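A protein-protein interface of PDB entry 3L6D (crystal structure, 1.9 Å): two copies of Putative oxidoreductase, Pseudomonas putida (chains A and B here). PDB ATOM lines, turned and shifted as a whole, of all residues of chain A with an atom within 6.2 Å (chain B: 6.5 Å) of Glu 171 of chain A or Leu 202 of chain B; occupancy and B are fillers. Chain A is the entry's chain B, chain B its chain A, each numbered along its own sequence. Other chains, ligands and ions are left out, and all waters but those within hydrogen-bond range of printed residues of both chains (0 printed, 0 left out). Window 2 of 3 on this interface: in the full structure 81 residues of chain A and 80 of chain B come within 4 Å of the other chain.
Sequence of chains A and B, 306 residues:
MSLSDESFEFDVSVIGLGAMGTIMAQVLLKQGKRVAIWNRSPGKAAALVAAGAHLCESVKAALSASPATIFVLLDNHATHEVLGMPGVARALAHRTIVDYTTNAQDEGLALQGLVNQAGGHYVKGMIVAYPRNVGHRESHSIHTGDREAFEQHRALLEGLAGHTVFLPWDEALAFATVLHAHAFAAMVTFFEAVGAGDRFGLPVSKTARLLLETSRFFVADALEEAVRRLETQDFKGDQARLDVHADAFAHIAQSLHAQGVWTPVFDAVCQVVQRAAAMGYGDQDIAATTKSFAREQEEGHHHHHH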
ATOM      1  N   LEU A 167      21.673  -5.986  -8.717  1.00  0.00           N
ATOM      2  CA  LEU A 167      21.191  -4.994  -7.800  1.00  0.00           C
ATOM      3  C   LEU A 167      19.657  -4.971  -7.895  1.00  0.00           C
ATOM      4  O   LEU A 167      19.099  -5.270  -8.968  1.00  0.00           O
ATOM      5  CB  LEU A 167      21.749  -3.604  -8.199  1.00  0.00           C
ATOM      6  CG  LEU A 167      23.264  -3.455  -8.054  1.00  0.00           C
ATOM      7  CD1 LEU A 167      23.697  -2.183  -8.751  1.00  0.00           C
ATOM      8  CD2 LEU A 167      23.581  -3.426  -6.559  1.00  0.00           C
ATOM      9  N   PRO A 168      18.976  -4.586  -6.797  1.00  0.00           N
ATOM     10  CA  PRO A 168      17.516  -4.468  -6.856  1.00  0.00           C
ATOM     11  C   PRO A 168      17.108  -3.340  -7.797  1.00  0.00           C
ATOM     12  O   PRO A 168      17.892  -2.398  -8.008  1.00  0.00           O
ATOM     13  CB  PRO A 168      17.121  -4.111  -5.392  1.00  0.00           C
ATOM     14  CG  PRO A 168      18.339  -3.503  -4.795  1.00  0.00           C
ATOM     15  CD  PRO A 168      19.515  -4.256  -5.456  1.00  0.00           C
ATOM     16  N   TRP A 169      15.890  -3.442  -8.334  1.00  0.00           N
ATOM     17  CA  TRP A 169      15.393  -2.594  -9.409  1.00  0.00           C
ATOM     18  C   TRP A 169      15.860  -1.114  -9.395  1.00  0.00           C
ATOM     19  O   TRP A 169      16.484  -0.617 -10.326  1.00  0.00           O
ATOM     20  CB  TRP A 169      13.848  -2.667  -9.477  1.00  0.00           C
ATOM     21  CG  TRP A 169      13.394  -2.174 -10.791  1.00  0.00           C
ATOM     22  CD1 TRP A 169      13.087  -0.871 -11.115  1.00  0.00           C
ATOM     23  CD2 TRP A 169      13.306  -2.931 -12.026  1.00  0.00           C
ATOM     24  NE1 TRP A 169      12.757  -0.791 -12.467  1.00  0.00           N
ATOM     25  CE2 TRP A 169      12.905  -2.036 -13.043  1.00  0.00           C
ATOM     26  CE3 TRP A 169      13.462  -4.277 -12.350  1.00  0.00           C
ATOM     27  CZ2 TRP A 169      12.679  -2.455 -14.378  1.00  0.00           C
ATOM     28  CZ3 TRP A 169      13.226  -4.690 -13.685  1.00  0.00           C
ATOM     29  CH2 TRP A 169      12.866  -3.778 -14.674  1.00  0.00           C
ATOM     30  N   ASP A 170      15.551  -0.402  -8.342  1.00  0.00           N
ATOM     31  CA  ASP A 170      15.789   1.014  -8.409  1.00  0.00           C
ATOM     32  C   ASP A 170      17.272   1.370  -8.294  1.00  0.00           C
ATOM     33  O   ASP A 170      17.739   2.342  -8.938  1.00  0.00           O
ATOM     34  CB  ASP A 170      14.903   1.705  -7.395  1.00  0.00           C
ATOM     35  CG  ASP A 170      13.425   1.512  -7.751  1.00  0.00           C
ATOM     36  OD1 ASP A 170      13.018   1.950  -8.865  1.00  0.00           O
ATOM     37  OD2 ASP A 170      12.708   0.841  -6.972  1.00  0.00           O
ATOM     38  N   GLU A 171      18.004   0.539  -7.547  1.00  0.00           N
ATOM     39  CA  GLU A 171      19.452   0.727  -7.474  1.00  0.00           C
ATOM     40  C   GLU A 171      20.114   0.387  -8.826  1.00  0.00           C
ATOM     41  O   GLU A 171      21.022   1.085  -9.263  1.00  0.00           O
ATOM     42  CB  GLU A 171      20.034  -0.125  -6.353  1.00  0.00           C
ATOM     43  CG  GLU A 171      19.564   0.373  -4.981  1.00  0.00           C
ATOM     44  CD  GLU A 171      20.227  -0.357  -3.847  1.00  0.00           C
ATOM     45  OE1 GLU A 171      21.048  -1.238  -4.113  1.00  0.00           O
ATOM     46  OE2 GLU A 171      19.909  -0.067  -2.665  1.00  0.00           O
ATOM     47  N   ALA A 172      19.651  -0.664  -9.476  1.00  0.00           N
ATOM     48  CA  ALA A 172      20.248  -1.048 -10.771  1.00  0.00           C
ATOM     49  C   ALA A 172      20.139   0.036 -11.833  1.00  0.00           C
ATOM     50  O   ALA A 172      21.124   0.359 -12.525  1.00  0.00           O
ATOM     51  CB  ALA A 172      19.663  -2.372 -11.294  1.00  0.00           C
ATOM     52  N   LEU A 173      18.958   0.628 -11.959  1.00  0.00           N
ATOM     53  CA  LEU A 173      18.765   1.648 -12.963  1.00  0.00           C
ATOM     54  C   LEU A 173      19.603   2.876 -12.663  1.00  0.00           C
ATOM     55  O   LEU A 173      20.254   3.421 -13.568  1.00  0.00           O
ATOM     56  CB  LEU A 173      17.281   2.046 -13.103  1.00  0.00           C
ATOM     57  CG  LEU A 173      16.369   0.872 -13.453  1.00  0.00           C
ATOM     58  CD1 LEU A 173      14.925   1.334 -13.515  1.00  0.00           C
ATOM     59  CD2 LEU A 173      16.804   0.273 -14.722  1.00  0.00           C
ATOM     60  N   ALA A 174      19.591   3.291 -11.397  1.00  0.00           N
ATOM     61  CA  ALA A 174      20.327   4.465 -10.943  1.00  0.00           C
ATOM     62  C   ALA A 174      21.820   4.233 -11.132  1.00  0.00           C
ATOM     63  O   ALA A 174      22.549   5.103 -11.654  1.00  0.00           O
ATOM     64  CB  ALA A 174      20.033   4.731  -9.444  1.00  0.00           C
ATOM     65  N   PHE A 175      22.276   3.061 -10.719  1.00  0.00           N
ATOM     66  CA  PHE A 175      23.694   2.795 -10.831  1.00  0.00           C
ATOM     67  C   PHE A 175      24.141   2.794 -12.302  1.00  0.00           C
ATOM     68  O   PHE A 175      25.210   3.305 -12.646  1.00  0.00           O
ATOM     69  CB  PHE A 175      24.047   1.473 -10.189  1.00  0.00           C
ATOM     70  CG  PHE A 175      25.506   1.158 -10.302  1.00  0.00           C
ATOM     71  CD1 PHE A 175      26.437   1.954  -9.634  1.00  0.00           C
ATOM     72  CD2 PHE A 175      25.938   0.094 -11.061  1.00  0.00           C
ATOM     73  CE1 PHE A 175      27.821   1.700  -9.744  1.00  0.00           C
ATOM     74  CE2 PHE A 175      27.314  -0.187 -11.187  1.00  0.00           C
ATOM     75  CZ  PHE A 175      28.260   0.637 -10.510  1.00  0.00           C
ATOM     76  N   ALA A 176      23.340   2.194 -13.168  1.00  0.00           N
ATOM     77  CA  ALA A 176      23.686   2.135 -14.580  1.00  0.00           C
ATOM     78  C   ALA A 176      23.704   3.541 -15.139  1.00  0.00           C
ATOM     79  O   ALA A 176      24.543   3.855 -15.966  1.00  0.00           O
ATOM     80  CB  ALA A 176      22.712   1.279 -15.354  1.00  0.00           C
ATOM     81  N   VAL A 178      24.425   6.543 -13.577  1.00  0.00           N
ATOM     82  CA  VAL A 178      25.573   7.289 -13.163  1.00  0.00           C
ATOM     83  C   VAL A 178      26.886   6.623 -13.648  1.00  0.00           C
ATOM     84  O   VAL A 178      27.864   7.329 -13.946  1.00  0.00           O
ATOM     85  CB  VAL A 178      25.552   7.525 -11.591  1.00  0.00           C
ATOM     86  CG1 VAL A 178      24.178   8.104 -11.176  1.00  0.00           C
ATOM     87  CG2 VAL A 178      25.822   6.254 -10.824  1.00  0.00           C
ATOM     88  N   VAL B 194      29.557  10.099  -8.832  1.00  0.00           N
ATOM     89  CA  VAL B 194      29.374   9.611  -7.474  1.00  0.00           C
ATOM     90  C   VAL B 194      28.378  10.505  -6.706  1.00  0.00           C
ATOM     91  O   VAL B 194      27.486   9.997  -6.001  1.00  0.00           O
ATOM     92  CB  VAL B 194      30.720   9.509  -6.743  1.00  0.00           C
ATOM     93  CG1 VAL B 194      30.520   9.284  -5.244  1.00  0.00           C
ATOM     94  CG2 VAL B 194      31.557   8.386  -7.383  1.00  0.00           C
ATOM     95  N   ALA B 196      26.019  12.287  -8.083  1.00  0.00           N
ATOM     96  CA  ALA B 196      24.708  11.957  -8.642  1.00  0.00           C
ATOM     97  C   ALA B 196      24.151  10.712  -7.996  1.00  0.00           C
ATOM     98  O   ALA B 196      22.972  10.678  -7.600  1.00  0.00           O
ATOM     99  CB  ALA B 196      24.776  11.768 -10.175  1.00  0.00           C
ATOM    100  N   GLY B 197      25.011   9.689  -7.843  1.00  0.00           N
ATOM    101  CA  GLY B 197      24.603   8.437  -7.226  1.00  0.00           C
ATOM    102  C   GLY B 197      24.029   8.664  -5.842  1.00  0.00           C
ATOM    103  O   GLY B 197      22.958   8.132  -5.496  1.00  0.00           O
ATOM    104  N   ASP B 198      24.736   9.469  -5.056  1.00  0.00           N
ATOM    105  CA  ASP B 198      24.252   9.820  -3.725  1.00  0.00           C
ATOM    106  C   ASP B 198      22.832  10.390  -3.756  1.00  0.00           C
ATOM    107  O   ASP B 198      22.003  10.093  -2.892  1.00  0.00           O
ATOM    108  CB  ASP B 198      25.198  10.796  -3.048  1.00  0.00           C
ATOM    109  CG  ASP B 198      24.639  11.311  -1.743  1.00  0.00           C
ATOM    110  OD1 ASP B 198      24.681  10.556  -0.756  1.00  0.00           O
ATOM    111  OD2 ASP B 198      24.108  12.447  -1.706  1.00  0.00           O
ATOM    112  N   ARG B 199      22.516  11.169  -4.775  1.00  0.00           N
ATOM    113  CA  ARG B 199      21.170  11.725  -4.827  1.00  0.00           C
ATOM    114  C   ARG B 199      20.100  10.734  -5.313  1.00  0.00           C
ATOM    115  O   ARG B 199      18.908  10.987  -5.195  1.00  0.00           O
ATOM    116  CB  ARG B 199      21.187  13.011  -5.642  1.00  0.00           C
ATOM    117  CG  ARG B 199      21.937  14.083  -4.883  1.00  0.00           C
ATOM    118  CD  ARG B 199      21.837  15.386  -5.550  1.00  0.00           C
ATOM    119  NE  ARG B 199      20.962  16.297  -4.834  1.00  0.00           N
ATOM    120  CZ  ARG B 199      21.034  17.618  -4.945  1.00  0.00           C
ATOM    121  NH1 ARG B 199      21.937  18.166  -5.753  1.00  0.00           N
ATOM    122  NH2 ARG B 199      20.207  18.390  -4.248  1.00  0.00           N
ATOM    123  N   PHE B 200      20.540   9.611  -5.866  1.00  0.00           N
ATOM    124  CA  PHE B 200      19.646   8.504  -6.139  1.00  0.00           C
ATOM    125  C   PHE B 200      19.502   7.598  -4.923  1.00  0.00           C
ATOM    126  O   PHE B 200      18.790   6.609  -4.991  1.00  0.00           O
ATOM    127  CB  PHE B 200      20.133   7.665  -7.321  1.00  0.00           C
ATOM    128  CG  PHE B 200      19.833   8.267  -8.688  1.00  0.00           C
ATOM    129  CD1 PHE B 200      20.815   8.956  -9.390  1.00  0.00           C
ATOM    130  CD2 PHE B 200      18.594   8.107  -9.281  1.00  0.00           C
ATOM    131  CE1 PHE B 200      20.553   9.505 -10.648  1.00  0.00           C
ATOM    132  CE2 PHE B 200      18.330   8.615 -10.534  1.00  0.00           C
ATOM    133  CZ  PHE B 200      19.304   9.339 -11.217  1.00  0.00           C
ATOM    134  N   GLY B 201      20.163   7.906  -3.819  1.00  0.00           N
ATOM    135  CA  GLY B 201      20.098   7.030  -2.648  1.00  0.00           C
ATOM    136  C   GLY B 201      21.163   5.925  -2.644  1.00  0.00           C
ATOM    137  O   GLY B 201      21.109   5.004  -1.839  1.00  0.00           O
ATOM    138  N   LEU B 202      22.149   6.016  -3.538  1.00  0.00           N
ATOM    139  CA  LEU B 202      23.249   5.053  -3.541  1.00  0.00           C
ATOM    140  C   LEU B 202      24.359   5.573  -2.657  1.00  0.00           C
ATOM    141  O   LEU B 202      24.970   6.590  -2.990  1.00  0.00           O
ATOM    142  CB  LEU B 202      23.802   4.818  -4.968  1.00  0.00           C
ATOM    143  CG  LEU B 202      22.809   4.571  -6.108  1.00  0.00           C
ATOM    144  CD1 LEU B 202      23.543   4.392  -7.424  1.00  0.00           C
ATOM    145  CD2 LEU B 202      21.870   3.357  -5.814  1.00  0.00           C
ATOM    146  N   PRO B 203      24.675   4.856  -1.571  1.00  0.00           N
ATOM    147  CA  PRO B 203      25.683   5.344  -0.602  1.00  0.00           C
ATOM    148  C   PRO B 203      27.067   5.478  -1.225  1.00  0.00           C
ATOM    149  O   PRO B 203      27.565   4.530  -1.847  1.00  0.00           O
ATOM    150  CB  PRO B 203      25.722   4.233   0.463  1.00  0.00           C
ATOM    151  CG  PRO B 203      25.298   2.987  -0.278  1.00  0.00           C
ATOM    152  CD  PRO B 203      24.265   3.462  -1.299  1.00  0.00           C
ATOM    153  N   VAL B 204      27.691   6.629  -1.015  1.00  0.00           N
ATOM    154  CA  VAL B 204      29.077   6.881  -1.449  1.00  0.00           C
ATOM    155  C   VAL B 204      30.044   5.762  -1.005  1.00  0.00           C
ATOM    156  O   VAL B 204      30.892   5.335  -1.782  1.00  0.00           O
ATOM    157  CB  VAL B 204      29.533   8.291  -0.994  1.00  0.00           C
ATOM    158  CG1 VAL B 204      31.048   8.431  -1.019  1.00  0.00           C
ATOM    159  CG2 VAL B 204      28.865   9.369  -1.851  1.00  0.00           C
ATOM    160  N   SER B 205      29.867   5.251   0.213  1.00  0.00           N
ATOM    161  CA  SER B 205      30.717   4.185   0.814  1.00  0.00           C
ATOM    162  C   SER B 205      30.890   2.871   0.021  1.00  0.00           C
ATOM    163  O   SER B 205      31.864   2.125   0.261  1.00  0.00           O
ATOM    164  CB  SER B 205      30.190   3.810   2.222  1.00  0.00           C
ATOM    165  OG  SER B 205      29.123   2.861   2.126  1.00  0.00           O
ATOM    166  N   THR B 207      29.339   2.815  -3.434  1.00  0.00           N
ATOM    167  CA  THR B 207      29.079   3.139  -4.838  1.00  0.00           C
ATOM    168  C   THR B 207      30.290   3.635  -5.592  1.00  0.00           C
ATOM    169  O   THR B 207      30.443   3.333  -6.787  1.00  0.00           O
ATOM    170  CB  THR B 207      27.886   4.078  -4.958  1.00  0.00           C
ATOM    171  OG1 THR B 207      26.823   3.498  -4.202  1.00  0.00           O
ATOM    172  CG2 THR B 207      27.457   4.244  -6.390  1.00  0.00           C
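No position is printed for both chains.
Glu 171 of chain A touches Leu 202 of chain B.
Ala 174 of chain A touches Phe 200 of chain B.
Phe 175 of chain A touches Leu 202 of chain B.
CB of Ala 196 of chain B touches CG1 of Val 178 of chain A (3.8 Å).
N of Gly 197 of chain B touches CG1 of Val 178 of chain A, 3.8 Å away.
CD1 of Phe 200 of chain B touches CG1 of Val 178 of chain A, at 3.9 Å.
Of chain A, only Glu 171 and Phe 175 come within 4 Å of Leu 202 of chain B.
Printed residues of chain A within 4 Å of Ala 196 of chain B: Val 178 (3.8 Å).
Printed residues of chain B within 4 Å of Ala 174 of chain A: Phe 200 (3.6 Å).
Of the printed residues of chain A, Gly 197 of chain B touches Val 178 (3.8 Å).
Printed residues of chain B within 4 Å of Phe 175 of chain A: Leu 202 (3.8 Å).
Printed residues of chain A within 4 Å of Phe 200 of chain B: Ala 174 (3.6 Å) and Val 178 (3.9 Å).
The nearest printed residue of chain B that does not touch Phe 175 of chain A is Thr 207 of chain B (4.1 Å).
Of the 11 printed residues of chain A, 4 touch a printed residue of chain B.
Printed residues of chain A that touch a printed residue of chain B: Glu 171, Ala 174, Phe 175 and Val 178.
Hydrophobic or aromatic side chains of chain A that line the printed part of chain B: Ala 174 and Val 178.
Along chain A the printed residues that touch a printed residue of chain B span positions 171 to 178.
Among the printed residues, 6 pairs touch across the chains.
Among the printed residues, no Asp or Glu carboxylate lies within 4 Å of a Lys or Arg side-chain nitrogen of the other chain.
The backbone carbonyl oxygen of Gly 197 of chain B is in hydrogen-bond range of the backbone NH of Leu 202 of chain B (3.0 Å).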
